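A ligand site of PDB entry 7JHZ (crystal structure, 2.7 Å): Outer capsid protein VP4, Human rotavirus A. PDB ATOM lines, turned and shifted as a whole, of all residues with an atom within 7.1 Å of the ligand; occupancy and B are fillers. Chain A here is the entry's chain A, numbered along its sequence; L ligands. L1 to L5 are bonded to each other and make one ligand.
An oxygen (O3) of LG5 L5 lies within hydrogen-bond range of the side-chain hydroxyl (OG1) of Thr 121 (2.6 Å).
The side-chain carboxylate of Asp 123 is in hydrogen-bond range of an oxygen (O1) of LIG L1, 3.0 Å away.
N of Thr 93 lies within hydrogen-bond range of O4 of LG2 L2, at 3.0 Å.
The backbone carbonyl oxygen (O) of Thr 93 lies within hydrogen-bond range of an oxygen (O4) of LG2 L2.
Merely in contact with the ligand: Arg 92, His 114, Gly 115, Glu 116 and Arg 119.
Within 4 Å of the ligand: Arg 92, Thr 93, His 114, Gly 115, Glu 116, Arg 119, Thr 121 and Asp 123.
O of Arg 92 sits at hydrogen-bond distance from ND2 of Asn 90 (2.8 Å).
The backbone carbonyl oxygen (O) of Thr 121 lies within hydrogen-bond range of the backbone NH (N) of His 114, at 2.8 Å.
O of Ser 124 lies within hydrogen-bond range of NH2 of Arg 92.
OG of Ser 125 is in hydrogen-bond range of NH2 of Arg 92 (2.9 Å).
N of Thr 95 sits at hydrogen-bond distance from O of Gly 115 (2.8 Å).
OG1 of Thr 93 lies within hydrogen-bond range of OD1 of Asn 90, 3.3 Å away.
The backbone carbonyl oxygen (O) of Thr 93 lies within hydrogen-bond range of the backbone NH (N) of Gly 115 (2.9 Å).
The side-chain carboxylate of Asp 123 lies within salt-bridge range of the guanidinium group of Arg 92.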
ATOM      1  N   LYS A  75      24.589 -17.409  27.091  1.00  0.00           N
ATOM      2  CA  LYS A  75      24.886 -15.954  27.107  1.00  0.00           C
ATOM      3  C   LYS A  75      25.794 -15.640  25.910  1.00  0.00           C
ATOM      4  O   LYS A  75      26.832 -16.264  25.785  1.00  0.00           O
ATOM      5  CB  LYS A  75      25.457 -15.516  28.454  1.00  0.00           C
ATOM      6  CG  LYS A  75      24.449 -15.322  29.570  1.00  0.00           C
ATOM      7  CD  LYS A  75      24.969 -14.392  30.671  1.00  0.00           C
ATOM      8  CE  LYS A  75      24.307 -14.569  32.021  1.00  0.00           C
ATOM      9  NZ  LYS A  75      22.837 -14.734  31.917  1.00  0.00           N
ATOM     10  N   LEU A  77      27.833 -12.752  24.586  1.00  0.00           N
ATOM     11  CA  LEU A  77      28.425 -11.440  24.967  1.00  0.00           C
ATOM     12  C   LEU A  77      28.913 -10.736  23.699  1.00  0.00           C
ATOM     13  O   LEU A  77      29.789 -11.261  22.986  1.00  0.00           O
ATOM     14  CB  LEU A  77      29.538 -11.674  25.994  1.00  0.00           C
ATOM     15  CG  LEU A  77      29.051 -12.289  27.306  1.00  0.00           C
ATOM     16  CD1 LEU A  77      30.184 -12.615  28.253  1.00  0.00           C
ATOM     17  CD2 LEU A  77      28.058 -11.367  27.985  1.00  0.00           C
ATOM     18  N   ASN A  90      32.203  -5.358  27.001  1.00  0.00           N
ATOM     19  CA  ASN A  90      30.915  -6.057  26.843  1.00  0.00           C
ATOM     20  C   ASN A  90      29.844  -5.004  26.651  1.00  0.00           C
ATOM     21  O   ASN A  90      29.370  -4.473  27.652  1.00  0.00           O
ATOM     22  CB  ASN A  90      30.640  -6.941  28.055  1.00  0.00           C
ATOM     23  CG  ASN A  90      29.344  -7.703  27.921  1.00  0.00           C
ATOM     24  OD1 ASN A  90      28.760  -8.116  28.927  1.00  0.00           O
ATOM     25  ND2 ASN A  90      28.895  -7.907  26.698  1.00  0.00           N
ATOM     26  N   ARG A  91      29.534  -4.665  25.399  1.00  0.00           N
ATOM     27  CA  ARG A  91      28.592  -3.585  25.042  1.00  0.00           C
ATOM     28  C   ARG A  91      27.153  -4.076  25.261  1.00  0.00           C
ATOM     29  O   ARG A  91      26.295  -3.289  25.692  1.00  0.00           O
ATOM     30  CB  ARG A  91      28.868  -3.201  23.589  1.00  0.00           C
ATOM     31  CG  ARG A  91      27.996  -2.072  23.091  1.00  0.00           C
ATOM     32  CD  ARG A  91      28.598  -1.428  21.869  1.00  0.00           C
ATOM     33  NE  ARG A  91      27.678  -0.424  21.367  1.00  0.00           N
ATOM     34  CZ  ARG A  91      27.890   0.321  20.286  1.00  0.00           C
ATOM     35  NH1 ARG A  91      29.010   0.162  19.590  1.00  0.00           N
ATOM     36  NH2 ARG A  91      26.996   1.207  19.910  1.00  0.00           N
ATOM     37  N   ARG A  92      26.877  -5.322  24.877  1.00  0.00           N
ATOM     38  CA  ARG A  92      25.507  -5.891  24.933  1.00  0.00           C
ATOM     39  C   ARG A  92      25.584  -7.357  25.327  1.00  0.00           C
ATOM     40  O   ARG A  92      26.626  -7.994  25.017  1.00  0.00           O
ATOM     41  CB  ARG A  92      24.825  -5.767  23.571  1.00  0.00           C
ATOM     42  CG  ARG A  92      24.341  -4.368  23.226  1.00  0.00           C
ATOM     43  CD  ARG A  92      23.551  -4.345  21.921  1.00  0.00           C
ATOM     44  NE  ARG A  92      23.645  -3.036  21.290  1.00  0.00           N
ATOM     45  CZ  ARG A  92      24.681  -2.616  20.567  1.00  0.00           C
ATOM     46  NH1 ARG A  92      25.736  -3.392  20.361  1.00  0.00           N
ATOM     47  NH2 ARG A  92      24.664  -1.403  20.060  1.00  0.00           N
ATOM     48  N   THR A  93      24.519  -7.892  25.898  1.00  0.00           N
ATOM     49  CA  THR A  93      24.373  -9.346  26.128  1.00  0.00           C
ATOM     50  C   THR A  93      23.026  -9.840  25.616  1.00  0.00           C
ATOM     51  O   THR A  93      21.999  -9.220  25.933  1.00  0.00           O
ATOM     52  CB  THR A  93      24.528  -9.673  27.617  1.00  0.00           C
ATOM     53  OG1 THR A  93      25.850  -9.299  28.023  1.00  0.00           O
ATOM     54  CG2 THR A  93      24.318 -11.140  27.949  1.00  0.00           C
ATOM     55  N   LEU A  94      23.018 -10.960  24.895  1.00  0.00           N
ATOM     56  CA  LEU A  94      21.824 -11.721  24.527  1.00  0.00           C
ATOM     57  C   LEU A  94      21.772 -13.006  25.360  1.00  0.00           C
ATOM     58  O   LEU A  94      22.662 -13.825  25.220  1.00  0.00           O
ATOM     59  CB  LEU A  94      21.870 -12.022  23.017  1.00  0.00           C
ATOM     60  CG  LEU A  94      20.783 -12.960  22.507  1.00  0.00           C
ATOM     61  CD1 LEU A  94      19.396 -12.387  22.821  1.00  0.00           C
ATOM     62  CD2 LEU A  94      20.956 -13.213  21.022  1.00  0.00           C
ATOM     63  N   THR A  95      20.730 -13.170  26.166  1.00  0.00           N
ATOM     64  CA  THR A  95      20.499 -14.377  26.987  1.00  0.00           C
ATOM     65  C   THR A  95      19.395 -15.190  26.317  1.00  0.00           C
ATOM     66  O   THR A  95      18.288 -14.663  26.191  1.00  0.00           O
ATOM     67  CB  THR A  95      20.173 -14.039  28.445  1.00  0.00           C
ATOM     68  OG1 THR A  95      21.237 -13.265  28.992  1.00  0.00           O
ATOM     69  CG2 THR A  95      19.985 -15.269  29.299  1.00  0.00           C
ATOM     70  N   PHE A 113      20.381  -8.342  18.226  1.00  0.00           N
ATOM     71  CA  PHE A 113      19.390  -8.575  19.305  1.00  0.00           C
ATOM     72  C   PHE A 113      20.132  -8.659  20.636  1.00  0.00           C
ATOM     73  O   PHE A 113      21.204  -9.243  20.650  1.00  0.00           O
ATOM     74  CB  PHE A 113      18.558  -9.829  19.023  1.00  0.00           C
ATOM     75  CG  PHE A 113      17.454  -9.602  18.025  1.00  0.00           C
ATOM     76  CD1 PHE A 113      17.681  -9.740  16.671  1.00  0.00           C
ATOM     77  CD2 PHE A 113      16.183  -9.237  18.449  1.00  0.00           C
ATOM     78  CE1 PHE A 113      16.657  -9.541  15.765  1.00  0.00           C
ATOM     79  CE2 PHE A 113      15.157  -9.024  17.540  1.00  0.00           C
ATOM     80  CZ  PHE A 113      15.399  -9.171  16.199  1.00  0.00           C
ATOM     81  N   HIS A 114      19.589  -8.010  21.664  1.00  0.00           N
ATOM     82  CA  HIS A 114      20.071  -8.140  23.055  1.00  0.00           C
ATOM     83  C   HIS A 114      18.894  -8.303  24.021  1.00  0.00           C
ATOM     84  O   HIS A 114      17.739  -8.211  23.614  1.00  0.00           O
ATOM     85  CB  HIS A 114      21.022  -6.996  23.423  1.00  0.00           C
ATOM     86  CG  HIS A 114      20.388  -5.681  23.673  1.00  0.00           C
ATOM     87  ND1 HIS A 114      19.311  -5.215  22.949  1.00  0.00           N
ATOM     88  CD2 HIS A 114      20.750  -4.672  24.496  1.00  0.00           C
ATOM     89  CE1 HIS A 114      19.002  -3.997  23.358  1.00  0.00           C
ATOM     90  NE2 HIS A 114      19.867  -3.648  24.294  1.00  0.00           N
ATOM     91  N   GLY A 115      19.217  -8.552  25.278  1.00  0.00           N
ATOM     92  CA  GLY A 115      18.250  -8.858  26.338  1.00  0.00           C
ATOM     93  C   GLY A 115      17.989 -10.334  26.408  1.00  0.00           C
ATOM     94  O   GLY A 115      18.867 -11.102  26.020  1.00  0.00           O
ATOM     95  N   GLU A 116      16.843 -10.747  26.925  1.00  0.00           N
ATOM     96  CA  GLU A 116      16.597 -12.160  27.305  1.00  0.00           C
ATOM     97  C   GLU A 116      15.406 -12.705  26.541  1.00  0.00           C
ATOM     98  O   GLU A 116      14.352 -12.119  26.672  1.00  0.00           O
ATOM     99  CB  GLU A 116      16.312 -12.282  28.795  1.00  0.00           C
ATOM    100  CG  GLU A 116      15.735 -13.635  29.131  1.00  0.00           C
ATOM    101  CD  GLU A 116      15.931 -14.130  30.545  1.00  0.00           C
ATOM    102  OE1 GLU A 116      16.547 -13.405  31.342  1.00  0.00           O
ATOM    103  OE2 GLU A 116      15.463 -15.253  30.844  1.00  0.00           O
ATOM    104  N   THR A 117      15.588 -13.781  25.771  1.00  0.00           N
ATOM    105  CA  THR A 117      14.490 -14.445  25.034  1.00  0.00           C
ATOM    106  C   THR A 117      13.456 -14.862  26.070  1.00  0.00           C
ATOM    107  O   THR A 117      13.855 -15.467  27.078  1.00  0.00           O
ATOM    108  CB  THR A 117      15.022 -15.603  24.174  1.00  0.00           C
ATOM    109  OG1 THR A 117      15.455 -16.646  25.046  1.00  0.00           O
ATOM    110  CG2 THR A 117      16.141 -15.193  23.254  1.00  0.00           C
ATOM    111  N   ARG A 119      11.854 -12.082  24.966  1.00  0.00           N
ATOM    112  CA  ARG A 119      11.678 -10.606  24.826  1.00  0.00           C
ATOM    113  C   ARG A 119      13.009  -9.915  24.489  1.00  0.00           C
ATOM    114  O   ARG A 119      13.196  -8.777  24.883  1.00  0.00           O
ATOM    115  CB  ARG A 119      11.125 -10.109  26.169  1.00  0.00           C
ATOM    116  CG  ARG A 119      10.037 -11.006  26.733  1.00  0.00           C
ATOM    117  CD  ARG A 119       9.450 -10.493  28.036  1.00  0.00           C
ATOM    118  NE  ARG A 119       8.995  -9.113  27.942  1.00  0.00           N
ATOM    119  CZ  ARG A 119       7.864  -8.698  27.378  1.00  0.00           C
ATOM    120  NH1 ARG A 119       7.014  -9.548  26.818  1.00  0.00           N
ATOM    121  NH2 ARG A 119       7.587  -7.403  27.365  1.00  0.00           N
ATOM    122  N   ALA A 120      13.874 -10.553  23.729  1.00  0.00           N
ATOM    123  CA  ALA A 120      15.081  -9.885  23.197  1.00  0.00           C
ATOM    124  C   ALA A 120      14.608  -8.841  22.178  1.00  0.00           C
ATOM    125  O   ALA A 120      13.695  -9.148  21.424  1.00  0.00           O
ATOM    126  CB  ALA A 120      16.045 -10.866  22.576  1.00  0.00           C
ATOM    127  N   THR A 121      15.249  -7.665  22.189  1.00  0.00           N
ATOM    128  CA  THR A 121      14.939  -6.555  21.257  1.00  0.00           C
ATOM    129  C   THR A 121      16.174  -6.202  20.433  1.00  0.00           C
ATOM    130  O   THR A 121      17.301  -6.551  20.818  1.00  0.00           O
ATOM    131  CB  THR A 121      14.381  -5.358  22.039  1.00  0.00           C
ATOM    132  OG1 THR A 121      15.249  -5.148  23.157  1.00  0.00           O
ATOM    133  CG2 THR A 121      12.961  -5.592  22.507  1.00  0.00           C
ATOM    134  N   THR A 122      15.940  -5.496  19.345  1.00  0.00           N
ATOM    135  CA  THR A 122      16.999  -5.071  18.405  1.00  0.00           C
ATOM    136  C   THR A 122      17.656  -3.776  18.938  1.00  0.00           C
ATOM    137  O   THR A 122      16.980  -2.991  19.616  1.00  0.00           O
ATOM    138  CB  THR A 122      16.475  -5.021  16.977  1.00  0.00           C
ATOM    139  OG1 THR A 122      17.630  -4.838  16.168  1.00  0.00           O
ATOM    140  CG2 THR A 122      15.467  -3.924  16.728  1.00  0.00           C
ATOM    141  N   ASP A 123      18.944  -3.610  18.683  1.00  0.00           N
ATOM    142  CA  ASP A 123      19.679  -2.376  19.024  1.00  0.00           C
ATOM    143  C   ASP A 123      20.666  -2.115  17.902  1.00  0.00           C
ATOM    144  O   ASP A 123      20.906  -3.033  17.103  1.00  0.00           O
ATOM    145  CB  ASP A 123      20.331  -2.473  20.402  1.00  0.00           C
ATOM    146  CG  ASP A 123      20.784  -1.140  20.969  1.00  0.00           C
ATOM    147  OD1 ASP A 123      20.108  -0.112  20.685  1.00  0.00           O
ATOM    148  OD2 ASP A 123      21.824  -1.142  21.676  1.00  0.00           O
ATOM    149  N   SER A 124      21.174  -0.898  17.825  1.00  0.00           N
ATOM    150  CA  SER A 124      21.984  -0.423  16.682  1.00  0.00           C
ATOM    151  C   SER A 124      23.349   0.048  17.173  1.00  0.00           C
ATOM    152  O   SER A 124      23.437   0.546  18.267  1.00  0.00           O
ATOM    153  CB  SER A 124      21.266   0.677  15.935  1.00  0.00           C
ATOM    154  OG  SER A 124      20.924   1.737  16.801  1.00  0.00           O
ATOM    155  N   SER A 125      24.363  -0.140  16.345  1.00  0.00           N
ATOM    156  CA  SER A 125      25.715   0.461  16.503  1.00  0.00           C
ATOM    157  C   SER A 125      25.965   1.297  15.256  1.00  0.00           C
ATOM    158  O   SER A 125      25.671   0.786  14.164  1.00  0.00           O
ATOM    159  CB  SER A 125      26.769  -0.608  16.666  1.00  0.00           C
ATOM    160  OG  SER A 125      26.533  -1.384  17.835  1.00  0.00           O
HETATM  161  C1  LIG L   1      22.482   0.349  24.494  1.00  0.00           C
HETATM  162  C2  LIG L   1      21.231  -0.472  24.916  1.00  0.00           C
HETATM  163  C3  LIG L   1      20.823  -0.282  26.356  1.00  0.00           C
HETATM  164  C4  LIG L   1      20.977   1.189  26.881  1.00  0.00           C
HETATM  165  C5  LIG L   1      22.038   1.989  26.100  1.00  0.00           C
HETATM  166  C6  LIG L   1      22.704   3.055  26.991  1.00  0.00           C
HETATM  167  O1  LIG L   1      23.522  -0.512  24.087  1.00  0.00           O
HETATM  168  O2  LIG L   1      20.078  -0.101  24.143  1.00  0.00           O
HETATM  169  O3  LIG L   1      21.638  -1.139  27.066  1.00  0.00           O
HETATM  170  O4  LIG L   1      21.271   1.152  28.312  1.00  0.00           O
HETATM  171  O5  LIG L   1      23.039   1.107  25.581  1.00  0.00           O
HETATM  172  O6  LIG L   1      22.816   4.303  26.287  1.00  0.00           O
HETATM  173  C1  LG2 L   2      21.185  -2.199  27.937  1.00  0.00           C
HETATM  174  C2  LG2 L   2      19.713  -2.674  28.079  1.00  0.00           C
HETATM  175  C3  LG2 L   2      19.801  -3.748  29.163  1.00  0.00           C
HETATM  176  C4  LG2 L   2      20.775  -4.862  28.713  1.00  0.00           C
HETATM  177  C5  LG2 L   2      22.107  -4.257  28.344  1.00  0.00           C
HETATM  178  C6  LG2 L   2      23.060  -5.248  27.684  1.00  0.00           C
HETATM  179  C7  LG2 L   2      17.802  -1.088  27.745  1.00  0.00           C
HETATM  180  C8  LG2 L   2      17.006   0.043  28.393  1.00  0.00           C
HETATM  181  N1  LG2 L   2      18.787  -1.610  28.528  1.00  0.00           N
HETATM  182  O1  LG2 L   2      18.534  -4.322  29.404  1.00  0.00           O
HETATM  183  O2  LG2 L   2      20.958  -5.821  29.777  1.00  0.00           O
HETATM  184  O3  LG2 L   2      21.877  -3.270  27.353  1.00  0.00           O
HETATM  185  O4  LG2 L   2      22.379  -6.012  26.673  1.00  0.00           O
HETATM  186  O5  LG2 L   2      17.567  -1.416  26.565  1.00  0.00           O
HETATM  187  C1  LG3 L   3      18.010  -4.123  30.765  1.00  0.00           C
HETATM  188  C2  LG3 L   3      16.584  -4.730  30.792  1.00  0.00           C
HETATM  189  C3  LG3 L   3      15.934  -4.562  32.140  1.00  0.00           C
HETATM  190  C4  LG3 L   3      16.805  -5.111  33.257  1.00  0.00           C
HETATM  191  C5  LG3 L   3      18.202  -4.477  33.208  1.00  0.00           C
HETATM  192  C6  LG3 L   3      18.963  -5.050  34.448  1.00  0.00           C
HETATM  193  O1  LG3 L   3      15.745  -4.071  29.836  1.00  0.00           O
HETATM  194  O2  LG3 L   3      14.774  -5.322  32.084  1.00  0.00           O
HETATM  195  O3  LG3 L   3      16.914  -6.564  33.124  1.00  0.00           O
HETATM  196  O4  LG3 L   3      18.831  -4.711  31.874  1.00  0.00           O
HETATM  197  O5  LG3 L   3      20.360  -4.709  34.432  1.00  0.00           O
HETATM  198  C1  LG4 L   4      21.006  -7.189  29.348  1.00  0.00           C
HETATM  199  C2  LG4 L   4      21.809  -7.986  30.339  1.00  0.00           C
HETATM  200  C3  LG4 L   4      21.070  -8.115  31.659  1.00  0.00           C
HETATM  201  C4  LG4 L   4      19.681  -8.712  31.480  1.00  0.00           C
HETATM  202  C5  LG4 L   4      18.906  -7.890  30.446  1.00  0.00           C
HETATM  203  C6  LG4 L   4      17.564  -8.576  30.105  1.00  0.00           C
HETATM  204  O1  LG4 L   4      23.068  -7.337  30.560  1.00  0.00           O
HETATM  205  O2  LG4 L   4      21.838  -8.969  32.500  1.00  0.00           O
HETATM  206  O3  LG4 L   4      19.815 -10.070  31.065  1.00  0.00           O
HETATM  207  O4  LG4 L   4      19.689  -7.741  29.223  1.00  0.00           O
HETATM  208  C1  LG5 L   5      14.978  -4.962  28.996  1.00  0.00           C
HETATM  209  C2  LG5 L   5      13.829  -4.182  28.290  1.00  0.00           C
HETATM  210  C3  LG5 L   5      14.401  -3.257  27.226  1.00  0.00           C
HETATM  211  C4  LG5 L   5      15.260  -4.107  26.242  1.00  0.00           C
HETATM  212  C5  LG5 L   5      16.403  -4.678  27.050  1.00  0.00           C
HETATM  213  C6  LG5 L   5      17.393  -5.413  26.133  1.00  0.00           C
HETATM  214  O1  LG5 L   5      13.076  -3.406  29.250  1.00  0.00           O
HETATM  215  O2  LG5 L   5      13.334  -2.574  26.553  1.00  0.00           O
HETATM  216  O3  LG5 L   5      14.499  -5.254  25.618  1.00  0.00           O
HETATM  217  O4  LG5 L   5      15.845  -5.591  28.017  1.00  0.00           O
